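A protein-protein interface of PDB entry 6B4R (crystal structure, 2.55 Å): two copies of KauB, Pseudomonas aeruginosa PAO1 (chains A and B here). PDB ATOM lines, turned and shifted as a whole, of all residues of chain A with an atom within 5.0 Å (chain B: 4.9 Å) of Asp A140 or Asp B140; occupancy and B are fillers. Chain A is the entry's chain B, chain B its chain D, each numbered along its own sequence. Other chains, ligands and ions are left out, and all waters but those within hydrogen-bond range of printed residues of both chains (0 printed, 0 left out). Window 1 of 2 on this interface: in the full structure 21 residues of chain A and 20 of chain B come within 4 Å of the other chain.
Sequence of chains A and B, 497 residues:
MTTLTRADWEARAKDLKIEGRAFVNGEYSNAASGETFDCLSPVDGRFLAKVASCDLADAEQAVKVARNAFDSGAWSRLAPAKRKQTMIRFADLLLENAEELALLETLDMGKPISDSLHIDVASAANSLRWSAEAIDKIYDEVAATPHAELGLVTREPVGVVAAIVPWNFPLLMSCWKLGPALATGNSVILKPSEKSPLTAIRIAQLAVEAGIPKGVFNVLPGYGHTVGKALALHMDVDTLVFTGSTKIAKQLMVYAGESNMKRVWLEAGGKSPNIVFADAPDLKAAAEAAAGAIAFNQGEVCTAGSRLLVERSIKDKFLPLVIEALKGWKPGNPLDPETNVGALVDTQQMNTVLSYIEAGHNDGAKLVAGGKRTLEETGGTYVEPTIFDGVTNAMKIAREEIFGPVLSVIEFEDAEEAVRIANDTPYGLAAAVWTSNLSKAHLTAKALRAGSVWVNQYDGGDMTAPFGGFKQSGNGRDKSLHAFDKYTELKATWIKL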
ATOM      1  N   ILE A 138     -27.616  27.182 -23.082  1.00  0.00           N
ATOM      2  CA  ILE A 138     -26.568  27.299 -22.078  1.00  0.00           C
ATOM      3  C   ILE A 138     -27.039  28.150 -20.910  1.00  0.00           C
ATOM      4  O   ILE A 138     -27.608  29.226 -21.099  1.00  0.00           O
ATOM      5  CB  ILE A 138     -25.289  27.924 -22.665  1.00  0.00           C
ATOM      6  CG1 ILE A 138     -24.793  27.106 -23.858  1.00  0.00           C
ATOM      7  CG2 ILE A 138     -24.203  28.026 -21.603  1.00  0.00           C
ATOM      8  CD1 ILE A 138     -23.649  27.754 -24.602  1.00  0.00           C
ATOM      9  N   TYR A 139     -26.799  27.660 -19.701  1.00  0.00           N
ATOM     10  CA  TYR A 139     -27.156  28.392 -18.499  1.00  0.00           C
ATOM     11  C   TYR A 139     -25.903  28.788 -17.730  1.00  0.00           C
ATOM     12  O   TYR A 139     -24.985  27.986 -17.576  1.00  0.00           O
ATOM     13  CB  TYR A 139     -28.079  27.548 -17.616  1.00  0.00           C
ATOM     14  CG  TYR A 139     -29.474  27.399 -18.177  1.00  0.00           C
ATOM     15  CD1 TYR A 139     -30.533  28.136 -17.663  1.00  0.00           C
ATOM     16  CD2 TYR A 139     -29.728  26.532 -19.232  1.00  0.00           C
ATOM     17  CE1 TYR A 139     -31.808  28.008 -18.180  1.00  0.00           C
ATOM     18  CE2 TYR A 139     -30.997  26.399 -19.757  1.00  0.00           C
ATOM     19  CZ  TYR A 139     -32.033  27.137 -19.228  1.00  0.00           C
ATOM     20  OH  TYR A 139     -33.297  27.000 -19.752  1.00  0.00           O
ATOM     21  N   ASP A 140     -25.862  30.033 -17.266  1.00  0.00           N
ATOM     22  CA  ASP A 140     -24.804  30.470 -16.363  1.00  0.00           C
ATOM     23  C   ASP A 140     -25.139  30.034 -14.937  1.00  0.00           C
ATOM     24  O   ASP A 140     -26.043  29.222 -14.726  1.00  0.00           O
ATOM     25  CB  ASP A 140     -24.599  31.983 -16.449  1.00  0.00           C
ATOM     26  CG  ASP A 140     -23.939  32.411 -17.753  1.00  0.00           C
ATOM     27  OD1 ASP A 140     -23.221  31.585 -18.363  1.00  0.00           O
ATOM     28  OD2 ASP A 140     -24.136  33.572 -18.171  1.00  0.00           O
ATOM     29  N   GLU A 141     -24.427  30.579 -13.958  1.00  0.00           N
ATOM     30  CA  GLU A 141     -24.489  30.027 -12.608  1.00  0.00           C
ATOM     31  C   GLU A 141     -24.895  31.008 -11.512  1.00  0.00           C
ATOM     32  O   GLU A 141     -24.605  32.202 -11.584  1.00  0.00           O
ATOM     33  CB  GLU A 141     -23.147  29.380 -12.257  1.00  0.00           C
ATOM     34  CG  GLU A 141     -22.732  28.283 -13.222  1.00  0.00           C
ATOM     35  CD  GLU A 141     -21.292  27.846 -13.037  1.00  0.00           C
ATOM     36  OE1 GLU A 141     -20.508  28.601 -12.423  1.00  0.00           O
ATOM     37  OE2 GLU A 141     -20.948  26.743 -13.509  1.00  0.00           O
ATOM     38  N   VAL A 142     -25.578  30.475 -10.503  1.00  0.00           N
ATOM     39  CA  VAL A 142     -25.844  31.183  -9.258  1.00  0.00           C
ATOM     40  C   VAL A 142     -25.172  30.416  -8.125  1.00  0.00           C
ATOM     41  O   VAL A 142     -25.457  29.238  -7.911  1.00  0.00           O
ATOM     42  CB  VAL A 142     -27.351  31.274  -8.962  1.00  0.00           C
ATOM     43  CG1 VAL A 142     -27.585  31.868  -7.579  1.00  0.00           C
ATOM     44  CG2 VAL A 142     -28.058  32.094 -10.026  1.00  0.00           C
ATOM     45  N   VAL A 153     -22.642  34.140 -11.589  1.00  0.00           N
ATOM     46  CA  VAL A 153     -21.458  33.793 -12.361  1.00  0.00           C
ATOM     47  C   VAL A 153     -21.846  33.689 -13.829  1.00  0.00           C
ATOM     48  O   VAL A 153     -22.316  32.646 -14.281  1.00  0.00           O
ATOM     49  CB  VAL A 153     -20.856  32.455 -11.903  1.00  0.00           C
ATOM     50  CG1 VAL A 153     -19.594  32.141 -12.692  1.00  0.00           C
ATOM     51  CG2 VAL A 153     -20.563  32.483 -10.408  1.00  0.00           C
ATOM     52  N   THR A 154     -21.651  34.774 -14.571  1.00  0.00           N
ATOM     53  CA  THR A 154     -22.134  34.855 -15.947  1.00  0.00           C
ATOM     54  C   THR A 154     -21.008  34.952 -16.977  1.00  0.00           C
ATOM     55  O   THR A 154     -19.847  35.165 -16.627  1.00  0.00           O
ATOM     56  CB  THR A 154     -23.097  36.046 -16.120  1.00  0.00           C
ATOM     57  OG1 THR A 154     -22.458  37.248 -15.673  1.00  0.00           O
ATOM     58  CG2 THR A 154     -24.363  35.824 -15.305  1.00  0.00           C
ATOM     59  N   ARG A 155     -21.362  34.786 -18.248  1.00  0.00           N
ATOM     60  CA  ARG A 155     -20.389  34.873 -19.333  1.00  0.00           C
ATOM     61  C   ARG A 155     -20.726  35.990 -20.320  1.00  0.00           C
ATOM     62  O   ARG A 155     -21.851  36.089 -20.803  1.00  0.00           O
ATOM     63  CB  ARG A 155     -20.271  33.535 -20.063  1.00  0.00           C
ATOM     64  CG  ARG A 155     -19.621  32.440 -19.233  1.00  0.00           C
ATOM     65  CD  ARG A 155     -19.405  31.175 -20.048  1.00  0.00           C
ATOM     66  NE  ARG A 155     -18.604  30.190 -19.326  1.00  0.00           N
ATOM     67  CZ  ARG A 155     -17.275  30.145 -19.346  1.00  0.00           C
ATOM     68  NH1 ARG A 155     -16.588  31.032 -20.055  1.00  0.00           N
ATOM     69  NH2 ARG A 155     -16.631  29.213 -18.656  1.00  0.00           N
ATOM     70  N   ILE B 138     -22.718  23.105  -5.203  1.00  0.00           N
ATOM     71  CA  ILE B 138     -23.817  23.089  -6.159  1.00  0.00           C
ATOM     72  C   ILE B 138     -24.125  24.505  -6.629  1.00  0.00           C
ATOM     73  O   ILE B 138     -24.218  25.428  -5.821  1.00  0.00           O
ATOM     74  CB  ILE B 138     -25.092  22.474  -5.540  1.00  0.00           C
ATOM     75  CG1 ILE B 138     -24.820  21.054  -5.044  1.00  0.00           C
ATOM     76  CG2 ILE B 138     -26.234  22.465  -6.546  1.00  0.00           C
ATOM     77  CD1 ILE B 138     -26.019  20.398  -4.390  1.00  0.00           C
ATOM     78  N   TYR B 139     -24.283  24.672  -7.937  1.00  0.00           N
ATOM     79  CA  TYR B 139     -24.617  25.972  -8.506  1.00  0.00           C
ATOM     80  C   TYR B 139     -25.977  25.947  -9.199  1.00  0.00           C
ATOM     81  O   TYR B 139     -26.268  25.044  -9.981  1.00  0.00           O
ATOM     82  CB  TYR B 139     -23.541  26.415  -9.501  1.00  0.00           C
ATOM     83  CG  TYR B 139     -22.226  26.803  -8.865  1.00  0.00           C
ATOM     84  CD1 TYR B 139     -21.888  28.136  -8.690  1.00  0.00           C
ATOM     85  CD2 TYR B 139     -21.324  25.835  -8.439  1.00  0.00           C
ATOM     86  CE1 TYR B 139     -20.691  28.499  -8.110  1.00  0.00           C
ATOM     87  CE2 TYR B 139     -20.120  26.189  -7.857  1.00  0.00           C
ATOM     88  CZ  TYR B 139     -19.808  27.524  -7.695  1.00  0.00           C
ATOM     89  OH  TYR B 139     -18.612  27.890  -7.115  1.00  0.00           O
ATOM     90  N   ASP B 140     -26.806  26.945  -8.909  1.00  0.00           N
ATOM     91  CA  ASP B 140     -28.070  27.123  -9.612  1.00  0.00           C
ATOM     92  C   ASP B 140     -27.833  27.800 -10.967  1.00  0.00           C
ATOM     93  O   ASP B 140     -26.690  27.920 -11.413  1.00  0.00           O
ATOM     94  CB  ASP B 140     -29.055  27.915  -8.751  1.00  0.00           C
ATOM     95  CG  ASP B 140     -29.576  27.107  -7.570  1.00  0.00           C
ATOM     96  OD1 ASP B 140     -29.739  25.876  -7.715  1.00  0.00           O
ATOM     97  OD2 ASP B 140     -29.820  27.698  -6.498  1.00  0.00           O
ATOM     98  N   GLU B 141     -28.904  28.249 -11.616  1.00  0.00           N
ATOM     99  CA  GLU B 141     -28.817  28.620 -13.027  1.00  0.00           C
ATOM    100  C   GLU B 141     -29.198  30.059 -13.364  1.00  0.00           C
ATOM    101  O   GLU B 141     -30.002  30.686 -12.676  1.00  0.00           O
ATOM    102  CB  GLU B 141     -29.646  27.648 -13.875  1.00  0.00           C
ATOM    103  CG  GLU B 141     -29.066  26.241 -13.945  1.00  0.00           C
ATOM    104  CD  GLU B 141     -30.057  25.226 -14.481  1.00  0.00           C
ATOM    105  OE1 GLU B 141     -31.260  25.346 -14.164  1.00  0.00           O
ATOM    106  OE2 GLU B 141     -29.636  24.310 -15.221  1.00  0.00           O
ATOM    107  N   VAL B 142     -28.598  30.567 -14.437  1.00  0.00           N
ATOM    108  CA  VAL B 142     -28.967  31.852 -15.021  1.00  0.00           C
ATOM    109  C   VAL B 142     -29.252  31.631 -16.503  1.00  0.00           C
ATOM    110  O   VAL B 142     -28.380  31.188 -17.248  1.00  0.00           O
ATOM    111  CB  VAL B 142     -27.839  32.895 -14.878  1.00  0.00           C
ATOM    112  CG1 VAL B 142     -28.262  34.227 -15.492  1.00  0.00           C
ATOM    113  CG2 VAL B 142     -27.454  33.079 -13.421  1.00  0.00           C
ATOM    114  N   VAL B 153     -32.777  30.760 -12.002  1.00  0.00           N
ATOM    115  CA  VAL B 153     -33.385  29.468 -11.706  1.00  0.00           C
ATOM    116  C   VAL B 153     -32.716  28.866 -10.472  1.00  0.00           C
ATOM    117  O   VAL B 153     -31.642  28.271 -10.568  1.00  0.00           O
ATOM    118  CB  VAL B 153     -33.258  28.492 -12.892  1.00  0.00           C
ATOM    119  CG1 VAL B 153     -33.954  27.179 -12.575  1.00  0.00           C
ATOM    120  CG2 VAL B 153     -33.830  29.109 -14.160  1.00  0.00           C
ATOM    121  N   THR B 154     -33.352  29.029  -9.314  1.00  0.00           N
ATOM    122  CA  THR B 154     -32.753  28.622  -8.043  1.00  0.00           C
ATOM    123  C   THR B 154     -33.522  27.497  -7.341  1.00  0.00           C
ATOM    124  O   THR B 154     -34.691  27.245  -7.638  1.00  0.00           O
ATOM    125  CB  THR B 154     -32.625  29.821  -7.080  1.00  0.00           C
ATOM    126  OG1 THR B 154     -33.929  30.326  -6.762  1.00  0.00           O
ATOM    127  CG2 THR B 154     -31.801  30.931  -7.715  1.00  0.00           C
ATOM    128  N   ARG B 155     -32.852  26.829  -6.404  1.00  0.00           N
ATOM    129  CA  ARG B 155     -33.464  25.750  -5.635  1.00  0.00           C
ATOM    130  C   ARG B 155     -33.625  26.130  -4.166  1.00  0.00           C
ATOM    131  O   ARG B 155     -32.724  26.710  -3.560  1.00  0.00           O
ATOM    132  CB  ARG B 155     -32.646  24.461  -5.763  1.00  0.00           C
ATOM    133  CG  ARG B 155     -32.662  23.865  -7.158  1.00  0.00           C
ATOM    134  CD  ARG B 155     -31.992  22.506  -7.196  1.00  0.00           C
ATOM    135  NE  ARG B 155     -32.156  21.857  -8.495  1.00  0.00           N
ATOM    136  CZ  ARG B 155     -33.195  21.096  -8.827  1.00  0.00           C
ATOM    137  NH1 ARG B 155     -34.172  20.884  -7.955  1.00  0.00           N
ATOM    138  NH2 ARG B 155     -33.258  20.545 -10.032  1.00  0.00           N
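O of Glu B141 is in hydrogen-bond range of N of Val B153. O of Glu A141 sits at hydrogen-bond distance from N of Val A153. The side-chain carboxylate (OD2) of Asp A140 lies within hydrogen-bond range of the backbone NH (N) of Arg A155 (3.0 Å). The side-chain carboxylate of Asp B140 is in hydrogen-bond range of the backbone NH of Arg B155, at 3.2 Å.
Tyr A139 touches Glu B141, and with the chains exchanged Glu A141 touches Tyr B139. Asp B140 touches its own counterpart, Asp A140. Asp A140 touches Glu B141, and with the chains exchanged Glu A141 touches Asp B140. Val B142 touches its own counterpart, Val A142. Positions printed for both chains: 138, 139, 140, 141, 142, 153, 154 and 155.
Of the printed residues of chain B, Asp A140 touches Asp B140, Glu B141 and Val B142. Of the printed residues of chain A, Asp B140 touches Asp A140 (3.6 Å), Glu A141 (3.3 Å) and Val A142 (2.8 Å). Printed residues of chain A within 4 Å of Glu B141: Tyr A139, Asp A140 and Val A142. Of the printed residues of chain A, Tyr B139 touches Glu A141 and Val A142. Arg B155 touches none of the printed residues of chain A. The nearest printed residue of chain A that does not touch Asp B140 is Tyr A139 (6.4 Å). The nearest printed residue of chain A that does not touch Tyr B139 is Val A153 (4.6 Å).
Of the 8 printed residues of chain B, 4 touch a printed residue of chain A. Of the 8 printed residues of chain A, 4 touch a printed residue of chain B. Hydrophobic or aromatic side chains of chain A within 4 Å of the printed part of chain B: Tyr A139 and Val A142. Among the printed residues, 12 pairs touch across the chains. Among the printed residues, no Asp or Glu carboxylate lies within 4 Å of a Lys or Arg side-chain nitrogen of the other chain.
N of Asp A140 lies within hydrogen-bond range of O of Val B142 (2.8 Å). The backbone NH (N) of Asp B140 is in hydrogen-bond range of the backbone carbonyl oxygen (O) of Val A142 (2.8 Å).
Among the printed residues, merely in contact across the chains: Glu A141 with Asp B140, Tyr A139 with Val B142, Asp A140 with Glu B141, Val A142 with Tyr B139, Glu A141 with Val B142, Val A142 with Glu B141, Val A142 with Val B142, Asp A140 with Asp B140, Tyr A139 with Glu B141 and Glu A141 with Tyr B139.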
